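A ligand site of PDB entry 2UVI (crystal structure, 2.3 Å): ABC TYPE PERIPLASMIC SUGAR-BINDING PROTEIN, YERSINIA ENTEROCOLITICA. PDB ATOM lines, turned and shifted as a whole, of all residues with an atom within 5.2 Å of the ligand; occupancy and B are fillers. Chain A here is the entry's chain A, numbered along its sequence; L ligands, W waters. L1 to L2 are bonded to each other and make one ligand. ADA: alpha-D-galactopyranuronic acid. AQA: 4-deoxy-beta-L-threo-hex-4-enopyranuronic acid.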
ATOM      1  N   TRP A  13      17.350   6.821  11.229  1.00  0.00           N
ATOM      2  CA  TRP A  13      18.406   7.019  12.228  1.00  0.00           C
ATOM      3  C   TRP A  13      17.891   6.633  13.619  1.00  0.00           C
ATOM      4  O   TRP A  13      16.688   6.567  13.851  1.00  0.00           O
ATOM      5  CB  TRP A  13      18.839   8.460  12.255  1.00  0.00           C
ATOM      6  CG  TRP A  13      17.858   9.315  13.002  1.00  0.00           C
ATOM      7  CD1 TRP A  13      17.850   9.562  14.338  1.00  0.00           C
ATOM      8  CD2 TRP A  13      16.732  10.032  12.447  1.00  0.00           C
ATOM      9  NE1 TRP A  13      16.802  10.414  14.659  1.00  0.00           N
ATOM     10  CE2 TRP A  13      16.099  10.701  13.527  1.00  0.00           C
ATOM     11  CE3 TRP A  13      16.217  10.187  11.144  1.00  0.00           C
ATOM     12  CZ2 TRP A  13      14.968  11.550  13.343  1.00  0.00           C
ATOM     13  CZ3 TRP A  13      15.111  10.977  10.950  1.00  0.00           C
ATOM     14  CH2 TRP A  13      14.482  11.639  12.053  1.00  0.00           C
ATOM     15  N   GLY A  14      18.787   6.380  14.534  1.00  0.00           N
ATOM     16  CA  GLY A  14      18.430   6.015  15.875  1.00  0.00           C
ATOM     17  C   GLY A  14      19.552   5.347  16.637  1.00  0.00           C
ATOM     18  O   GLY A  14      20.690   5.240  16.126  1.00  0.00           O
ATOM     19  N   ARG A  18      16.795   0.834  18.539  1.00  0.00           N
ATOM     20  CA  ARG A  18      15.813   1.204  17.499  1.00  0.00           C
ATOM     21  C   ARG A  18      16.118   0.550  16.191  1.00  0.00           C
ATOM     22  O   ARG A  18      15.205   0.179  15.481  1.00  0.00           O
ATOM     23  CB  ARG A  18      15.669   2.740  17.348  1.00  0.00           C
ATOM     24  CG  ARG A  18      14.826   3.208  16.142  1.00  0.00           C
ATOM     25  CD  ARG A  18      14.910   4.702  15.905  1.00  0.00           C
ATOM     26  NE  ARG A  18      14.452   5.416  17.082  1.00  0.00           N
ATOM     27  CZ  ARG A  18      14.314   6.725  17.169  1.00  0.00           C
ATOM     28  NH1 ARG A  18      14.670   7.495  16.168  1.00  0.00           N
ATOM     29  NH2 ARG A  18      13.903   7.284  18.290  1.00  0.00           N
ATOM     30  N   TRP A  45      22.065   9.485  14.511  1.00  0.00           N
ATOM     31  CA  TRP A  45      21.671  10.840  14.114  1.00  0.00           C
ATOM     32  C   TRP A  45      22.799  11.581  13.356  1.00  0.00           C
ATOM     33  O   TRP A  45      22.533  12.384  12.463  1.00  0.00           O
ATOM     34  CB  TRP A  45      21.240  11.675  15.362  1.00  0.00           C
ATOM     35  CG  TRP A  45      20.972  13.109  15.026  1.00  0.00           C
ATOM     36  CD1 TRP A  45      21.702  14.223  15.403  1.00  0.00           C
ATOM     37  CD2 TRP A  45      19.893  13.598  14.184  1.00  0.00           C
ATOM     38  NE1 TRP A  45      21.128  15.379  14.859  1.00  0.00           N
ATOM     39  CE2 TRP A  45      20.018  15.021  14.112  1.00  0.00           C
ATOM     40  CE3 TRP A  45      18.800  12.984  13.528  1.00  0.00           C
ATOM     41  CZ2 TRP A  45      19.116  15.798  13.393  1.00  0.00           C
ATOM     42  CZ3 TRP A  45      17.914  13.765  12.795  1.00  0.00           C
ATOM     43  CH2 TRP A  45      18.068  15.154  12.738  1.00  0.00           C
ATOM     44  N   ASN A  68      12.527  14.263   9.616  1.00  0.00           N
ATOM     45  CA  ASN A  68      12.431  15.154  10.748  1.00  0.00           C
ATOM     46  C   ASN A  68      11.538  16.306  10.333  1.00  0.00           C
ATOM     47  O   ASN A  68      11.473  16.676   9.174  1.00  0.00           O
ATOM     48  CB  ASN A  68      13.803  15.630  11.242  1.00  0.00           C
ATOM     49  CG  ASN A  68      13.970  15.488  12.742  1.00  0.00           C
ATOM     50  OD1 ASN A  68      13.331  14.628  13.392  1.00  0.00           O
ATOM     51  ND2 ASN A  68      14.804  16.351  13.336  1.00  0.00           N
ATOM     52  N   THR A 119       6.907  14.897  20.854  1.00  0.00           N
ATOM     53  CA  THR A 119       7.976  14.893  21.842  1.00  0.00           C
ATOM     54  C   THR A 119       8.256  16.319  22.292  1.00  0.00           C
ATOM     55  O   THR A 119       7.972  17.201  21.592  1.00  0.00           O
ATOM     56  CB  THR A 119       9.267  14.200  21.245  1.00  0.00           C
ATOM     57  OG1 THR A 119      10.159  13.863  22.312  1.00  0.00           O
ATOM     58  CG2 THR A 119       9.999  15.109  20.171  1.00  0.00           C
ATOM     59  N   ARG A 121      11.707  18.299  24.574  1.00  0.00           N
ATOM     60  CA  ARG A 121      12.903  18.092  25.445  1.00  0.00           C
ATOM     61  C   ARG A 121      12.523  18.255  26.930  1.00  0.00           C
ATOM     62  O   ARG A 121      11.890  19.215  27.278  1.00  0.00           O
ATOM     63  CB  ARG A 121      14.027  19.065  25.097  1.00  0.00           C
ATOM     64  CG  ARG A 121      14.724  18.835  23.771  1.00  0.00           C
ATOM     65  CD  ARG A 121      16.058  19.571  23.718  1.00  0.00           C
ATOM     66  NE  ARG A 121      16.712  19.427  22.417  1.00  0.00           N
ATOM     67  CZ  ARG A 121      17.505  18.407  22.085  1.00  0.00           C
ATOM     68  NH1 ARG A 121      17.798  17.442  22.966  1.00  0.00           N
ATOM     69  NH2 ARG A 121      18.009  18.340  20.866  1.00  0.00           N
ATOM     70  N   GLU A 165      24.643  18.989  25.006  1.00  0.00           N
ATOM     71  CA  GLU A 165      25.228  19.229  23.688  1.00  0.00           C
ATOM     72  C   GLU A 165      24.701  20.547  23.222  1.00  0.00           C
ATOM     73  O   GLU A 165      23.654  20.957  23.677  1.00  0.00           O
ATOM     74  CB  GLU A 165      24.871  18.140  22.725  1.00  0.00           C
ATOM     75  CG  GLU A 165      25.361  16.801  23.143  1.00  0.00           C
ATOM     76  CD  GLU A 165      25.003  15.764  22.127  1.00  0.00           C
ATOM     77  OE1 GLU A 165      25.683  15.740  21.114  1.00  0.00           O
ATOM     78  OE2 GLU A 165      24.026  14.985  22.342  1.00  0.00           O
ATOM     79  N   GLN A 167      23.036  21.744  20.790  1.00  0.00           N
ATOM     80  CA  GLN A 167      21.628  21.830  20.383  1.00  0.00           C
ATOM     81  C   GLN A 167      20.658  21.788  21.566  1.00  0.00           C
ATOM     82  O   GLN A 167      19.589  22.441  21.514  1.00  0.00           O
ATOM     83  CB  GLN A 167      21.310  20.708  19.399  1.00  0.00           C
ATOM     84  CG  GLN A 167      19.925  20.755  18.862  1.00  0.00           C
ATOM     85  CD  GLN A 167      19.698  19.682  17.850  1.00  0.00           C
ATOM     86  OE1 GLN A 167      20.232  18.544  17.943  1.00  0.00           O
ATOM     87  NE2 GLN A 167      18.878  20.010  16.865  1.00  0.00           N
ATOM     88  N   ASP A 168      21.030  21.020  22.593  1.00  0.00           N
ATOM     89  CA  ASP A 168      20.272  20.838  23.867  1.00  0.00           C
ATOM     90  C   ASP A 168      20.226  22.144  24.547  1.00  0.00           C
ATOM     91  O   ASP A 168      19.156  22.597  24.929  1.00  0.00           O
ATOM     92  CB  ASP A 168      20.941  19.862  24.826  1.00  0.00           C
ATOM     93  CG  ASP A 168      21.259  18.521  24.196  1.00  0.00           C
ATOM     94  OD1 ASP A 168      21.919  17.716  24.892  1.00  0.00           O
ATOM     95  OD2 ASP A 168      20.828  18.259  23.031  1.00  0.00           O
ATOM     96  N   MET A 246      16.432  16.220  27.055  1.00  0.00           N
ATOM     97  CA  MET A 246      16.280  15.254  25.974  1.00  0.00           C
ATOM     98  C   MET A 246      14.856  14.921  25.581  1.00  0.00           C
ATOM     99  O   MET A 246      13.983  14.858  26.418  1.00  0.00           O
ATOM    100  CB  MET A 246      17.016  13.981  26.343  1.00  0.00           C
ATOM    101  CG  MET A 246      17.174  12.986  25.168  1.00  0.00           C
ATOM    102  SD  MET A 246      18.011  13.594  23.701  1.00  0.00           S
ATOM    103  CE  MET A 246      19.507  14.306  24.435  1.00  0.00           C
ATOM    104  N   TRP A 247      14.646  14.746  24.283  1.00  0.00           N
ATOM    105  CA  TRP A 247      13.399  14.148  23.715  1.00  0.00           C
ATOM    106  C   TRP A 247      13.012  12.881  24.405  1.00  0.00           C
ATOM    107  O   TRP A 247      13.822  11.970  24.463  1.00  0.00           O
ATOM    108  CB  TRP A 247      13.640  13.783  22.221  1.00  0.00           C
ATOM    109  CG  TRP A 247      14.229  14.871  21.455  1.00  0.00           C
ATOM    110  CD1 TRP A 247      15.446  14.887  20.859  1.00  0.00           C
ATOM    111  CD2 TRP A 247      13.627  16.170  21.207  1.00  0.00           C
ATOM    112  NE1 TRP A 247      15.647  16.112  20.244  1.00  0.00           N
ATOM    113  CE2 TRP A 247      14.539  16.913  20.443  1.00  0.00           C
ATOM    114  CE3 TRP A 247      12.425  16.764  21.587  1.00  0.00           C
ATOM    115  CZ2 TRP A 247      14.294  18.260  20.059  1.00  0.00           C
ATOM    116  CZ3 TRP A 247      12.130  18.092  21.155  1.00  0.00           C
ATOM    117  CH2 TRP A 247      13.074  18.822  20.416  1.00  0.00           C
ATOM    118  N   SER A 249      11.207  10.758  23.044  1.00  0.00           N
ATOM    119  CA  SER A 249      11.064   9.796  21.941  1.00  0.00           C
ATOM    120  C   SER A 249      12.266   8.900  21.668  1.00  0.00           C
ATOM    121  O   SER A 249      12.166   7.993  20.851  1.00  0.00           O
ATOM    122  CB  SER A 249      10.774  10.573  20.663  1.00  0.00           C
ATOM    123  OG  SER A 249      11.938  11.278  20.251  1.00  0.00           O
ATOM    124  N   THR A 250      13.388   9.179  22.337  1.00  0.00           N
ATOM    125  CA  THR A 250      14.662   8.529  22.121  1.00  0.00           C
ATOM    126  C   THR A 250      15.468   8.526  23.389  1.00  0.00           C
ATOM    127  O   THR A 250      16.715   8.320  23.361  1.00  0.00           O
ATOM    128  CB  THR A 250      15.474   9.149  20.974  1.00  0.00           C
ATOM    129  OG1 THR A 250      16.555   8.274  20.623  1.00  0.00           O
ATOM    130  CG2 THR A 250      15.961  10.586  21.263  1.00  0.00           C
ATOM    131  N   LYS A 253      17.976   5.504  24.210  1.00  0.00           N
ATOM    132  CA  LYS A 253      19.275   5.557  23.565  1.00  0.00           C
ATOM    133  C   LYS A 253      20.337   6.014  24.573  1.00  0.00           C
ATOM    134  O   LYS A 253      21.538   5.751  24.411  1.00  0.00           O
ATOM    135  CB  LYS A 253      19.196   6.509  22.339  1.00  0.00           C
ATOM    136  CG  LYS A 253      20.516   6.716  21.594  1.00  0.00           C
ATOM    137  CD  LYS A 253      20.339   7.325  20.200  1.00  0.00           C
ATOM    138  CE  LYS A 253      20.186   8.852  20.274  1.00  0.00           C
ATOM    139  NZ  LYS A 253      20.070   9.482  18.891  1.00  0.00           N
ATOM    140  N   TYR A 254      19.870   6.769  25.570  1.00  0.00           N
ATOM    141  CA  TYR A 254      20.671   7.327  26.667  1.00  0.00           C
ATOM    142  C   TYR A 254      20.725   6.346  27.876  1.00  0.00           C
ATOM    143  O   TYR A 254      21.806   5.818  28.229  1.00  0.00           O
ATOM    144  CB  TYR A 254      20.181   8.766  27.021  1.00  0.00           C
ATOM    145  CG  TYR A 254      20.365   9.671  25.826  1.00  0.00           C
ATOM    146  CD1 TYR A 254      21.580  10.297  25.611  1.00  0.00           C
ATOM    147  CD2 TYR A 254      19.385   9.758  24.825  1.00  0.00           C
ATOM    148  CE1 TYR A 254      21.808  11.062  24.442  1.00  0.00           C
ATOM    149  CE2 TYR A 254      19.606  10.526  23.663  1.00  0.00           C
ATOM    150  CZ  TYR A 254      20.830  11.180  23.494  1.00  0.00           C
ATOM    151  OH  TYR A 254      21.107  11.913  22.376  1.00  0.00           O
ATOM    152  N   LYS A 283       6.840  18.991  19.134  1.00  0.00           N
ATOM    153  CA  LYS A 283       6.807  18.796  17.701  1.00  0.00           C
ATOM    154  C   LYS A 283       6.662  17.303  17.426  1.00  0.00           C
ATOM    155  O   LYS A 283       6.834  16.476  18.365  1.00  0.00           O
ATOM    156  CB  LYS A 283       8.138  19.325  17.083  1.00  0.00           C
ATOM    157  CG  LYS A 283       9.380  18.638  17.708  1.00  0.00           C
ATOM    158  CD  LYS A 283      10.607  18.866  16.914  1.00  0.00           C
ATOM    159  CE  LYS A 283      11.757  18.003  17.324  1.00  0.00           C
ATOM    160  NZ  LYS A 283      12.988  18.474  16.621  1.00  0.00           N
ATOM    161  N   PRO A 284       6.320  16.941  16.153  1.00  0.00           N
ATOM    162  CA  PRO A 284       6.534  15.567  15.685  1.00  0.00           C
ATOM    163  C   PRO A 284       7.987  15.079  15.983  1.00  0.00           C
ATOM    164  O   PRO A 284       8.946  15.756  15.650  1.00  0.00           O
ATOM    165  CB  PRO A 284       6.222  15.650  14.156  1.00  0.00           C
ATOM    166  CG  PRO A 284       5.092  16.785  14.119  1.00  0.00           C
ATOM    167  CD  PRO A 284       5.621  17.781  15.154  1.00  0.00           C
ATOM    168  N   ALA A 285       8.117  13.892  16.607  1.00  0.00           N
ATOM    169  CA  ALA A 285       9.410  13.415  17.078  1.00  0.00           C
ATOM    170  C   ALA A 285      10.164  12.979  15.820  1.00  0.00           C
ATOM    171  O   ALA A 285      11.415  13.177  15.680  1.00  0.00           O
ATOM    172  CB  ALA A 285       9.217  12.274  17.930  1.00  0.00           C
ATOM    173  N   GLN A 286       9.396  12.330  14.936  1.00  0.00           N
ATOM    174  CA  GLN A 286       9.763  12.127  13.559  1.00  0.00           C
ATOM    175  C   GLN A 286       8.610  11.601  12.756  1.00  0.00           C
ATOM    176  O   GLN A 286       7.537  11.310  13.315  1.00  0.00           O
ATOM    177  CB  GLN A 286      10.930  11.145  13.453  1.00  0.00           C
ATOM    178  CG  GLN A 286      10.555   9.847  13.876  1.00  0.00           C
ATOM    179  CD  GLN A 286      11.092   9.565  15.132  1.00  0.00           C
ATOM    180  OE1 GLN A 286      10.369   9.232  16.075  1.00  0.00           O
ATOM    181  NE2 GLN A 286      12.390   9.626  15.206  1.00  0.00           N
ATOM    182  N   ARG A 321      10.462   4.764  19.342  1.00  0.00           N
ATOM    183  CA  ARG A 321      10.285   6.063  18.653  1.00  0.00           C
ATOM    184  C   ARG A 321       9.389   7.033  19.445  1.00  0.00           C
ATOM    185  O   ARG A 321       9.078   8.162  18.985  1.00  0.00           O
ATOM    186  CB  ARG A 321       9.814   5.870  17.200  1.00  0.00           C
ATOM    187  CG  ARG A 321      10.999   5.391  16.294  1.00  0.00           C
ATOM    188  CD  ARG A 321      10.486   4.937  14.948  1.00  0.00           C
ATOM    189  NE  ARG A 321      11.468   4.599  13.915  1.00  0.00           N
ATOM    190  CZ  ARG A 321      11.927   3.373  13.670  1.00  0.00           C
ATOM    191  NH1 ARG A 321      11.585   2.371  14.441  1.00  0.00           N
ATOM    192  NH2 ARG A 321      12.765   3.165  12.674  1.00  0.00           N
ATOM    193  N   ASP A 366      15.216  25.415  14.367  1.00  0.00           N
ATOM    194  CA  ASP A 366      16.020  24.199  14.281  1.00  0.00           C
ATOM    195  C   ASP A 366      16.666  23.994  12.919  1.00  0.00           C
ATOM    196  O   ASP A 366      16.867  22.871  12.503  1.00  0.00           O
ATOM    197  CB  ASP A 366      15.184  22.988  14.609  1.00  0.00           C
ATOM    198  CG  ASP A 366      15.976  21.855  15.184  1.00  0.00           C
ATOM    199  OD1 ASP A 366      16.925  22.094  15.956  1.00  0.00           O
ATOM    200  OD2 ASP A 366      15.602  20.683  14.942  1.00  0.00           O
HETATM  201  C1  ADA L   1      19.020  14.516  20.019  1.00  0.00           C
HETATM  202  C2  ADA L   1      18.676  13.133  19.451  1.00  0.00           C
HETATM  203  C3  ADA L   1      18.851  13.084  17.910  1.00  0.00           C
HETATM  204  C4  ADA L   1      18.174  14.235  17.162  1.00  0.00           C
HETATM  205  C5  ADA L   1      18.814  15.477  17.744  1.00  0.00           C
HETATM  206  C6  ADA L   1      18.075  16.683  17.229  1.00  0.00           C
HETATM  207  O1  ADA L   1      20.328  14.604  19.908  1.00  0.00           O
HETATM  208  O2  ADA L   1      19.520  12.162  20.061  1.00  0.00           O
HETATM  209  O3  ADA L   1      18.360  11.882  17.368  1.00  0.00           O
HETATM  210  O4  ADA L   1      16.786  14.400  17.374  1.00  0.00           O
HETATM  211  O5  ADA L   1      18.657  15.660  19.188  1.00  0.00           O
HETATM  212  O6B ADA L   1      17.284  17.256  18.006  1.00  0.00           O
HETATM  213  O6A ADA L   1      18.280  17.029  16.067  1.00  0.00           O
HETATM  214  O6A AQA L   2      15.491   9.963  17.358  1.00  0.00           O
HETATM  215  C6  AQA L   2      14.557  10.686  17.779  1.00  0.00           C
HETATM  216  O6B AQA L   2      13.583  10.273  18.464  1.00  0.00           O
HETATM  217  C5  AQA L   2      14.663  12.147  17.440  1.00  0.00           C
HETATM  218  O5  AQA L   2      15.782  12.505  16.676  1.00  0.00           O
HETATM  219  C4  AQA L   2      13.576  13.106  17.905  1.00  0.00           C
HETATM  220  C3  AQA L   2      13.859  14.557  17.595  1.00  0.00           C
HETATM  221  O3  AQA L   2      12.580  15.167  17.301  1.00  0.00           O
HETATM  222  C2  AQA L   2      14.749  14.757  16.336  1.00  0.00           C
HETATM  223  O2  AQA L   2      15.126  16.135  16.129  1.00  0.00           O
HETATM  224  C1  AQA L   2      15.994  13.887  16.362  1.00  0.00           C
HETATM  225  O   HOH W   1      15.354  19.349  17.333  1.00  0.00           O
HETATM  226  O   HOH W   2      21.611  16.131  21.677  1.00  0.00           O
HETATM  227  O   HOH W   3      17.326  18.498  14.150  1.00  0.00           O
HETATM  228  O   HOH W   4      17.941   8.514  18.045  1.00  0.00           O
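The side-chain hydroxyl (OG) of Ser 249 lies within hydrogen-bond range of an oxygen (O6B) of AQA L2 (2.6 Å). The side-chain hydroxyl (OH) of Tyr 254 lies within hydrogen-bond range of an oxygen (O2) of ADA L1 (2.8 Å). The backbone carbonyl oxygen of Ala 285 is in hydrogen-bond range of an oxygen (O3) of AQA L2, 2.8 Å away. The side-chain amide nitrogen (ND2) of Asn 68 is in hydrogen-bond range of an oxygen (O2) of AQA L2, at 2.8 Å. NH1 of Arg 18 lies within salt-bridge range of O6A of AQA L2, at 2.9 Å. O6A of ADA L1 sits close to OE1 of Gln 167, at 3.1 Å. The side-chain amino group (NZ) of Lys 283 lies within hydrogen-bond range of an oxygen (O2) of AQA L2 (3.2 Å). The side-chain amino group (NZ) of Lys 253 sits at hydrogen-bond distance from an oxygen (O2) of ADA L1, 3.0 Å away. NE1 of Trp 247 sits at hydrogen-bond distance from O6B of ADA L1. An oxygen (O6A) of AQA L2 sits at hydrogen-bond distance from the indole nitrogen (NE1) of Trp 13 (3.0 Å). The guanidinium group (NH2) of Arg 121 lies within salt-bridge range of an oxygen (O6B) of ADA L1, 3.1 Å away.
NH2 of Arg 18 is in hydrogen-bond range of O of Ser 249 (3.2 Å). The backbone NH (N) of Ser 249 is in hydrogen-bond range of the side-chain hydroxyl (OG1) of Thr 119 (3.4 Å). The side-chain sulfur (SD) of Met 246 sits close to the side-chain hydroxyl (OH) of Tyr 254 (3.8 Å). O of Ala 285 lies close to OD1 of Asn 68. The guanidinium group (NH1) of Arg 18 sits close to the side-chain amide nitrogen (NE2) of Gln 286 (3.3 Å). N of Thr 119 is in hydrogen-bond range of O of Lys 283, 2.9 Å away. OD2 of Asp 366 lies within salt-bridge range of NZ of Lys 283 (3.8 Å). OE1 of Gln 286 lies close to O of Arg 321.
CZ2 of Trp 45 touches O6A of ADA L1 (3.1 Å). CG2 of Thr 119 touches O3 of AQA L2 (3.9 Å). SD of Met 246 touches C1 of ADA L1 (3.9 Å). Thr 250 touches the ligand. NE2 of Gln 286 touches C6 of AQA L2 (3.5 Å). Hydrophobic or aromatic side chains that line the ligand: Trp 13, Trp 45, Met 246, Trp 247 and Tyr 254. Of the 22 residues printed, 16 come within 4 Å of the ligand. The nearest printed residue that does not touch the ligand is Pro 284 (4.03 Å).
Water W3 lies within hydrogen-bond range of O6A of ADA L1 (2.6 Å), OD2 of Asp 366 (2.9 Å), ND2 of Asn 68 (3.4 Å) and NE2 of Gln 167 (3.5 Å). Water W2 lies within hydrogen-bond range of the side-chain carboxylate (OD2) of Asp 168 (2.6 Å), an oxygen (O1) of ADA L1 (2.7 Å) and the side-chain carboxylate (OE2) of Glu 165 (2.8 Å). Water W1 lies within hydrogen-bond range of NZ of Lys 283 (2.6 Å), OD2 of Asp 366 (2.7 Å) and O6B of ADA L1 (2.9 Å). Water W4 lies within hydrogen-bond range of NZ of Lys 253 (2.5 Å), O6A of AQA L2 (2.9 Å) and OG1 of Thr 250 (2.9 Å).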
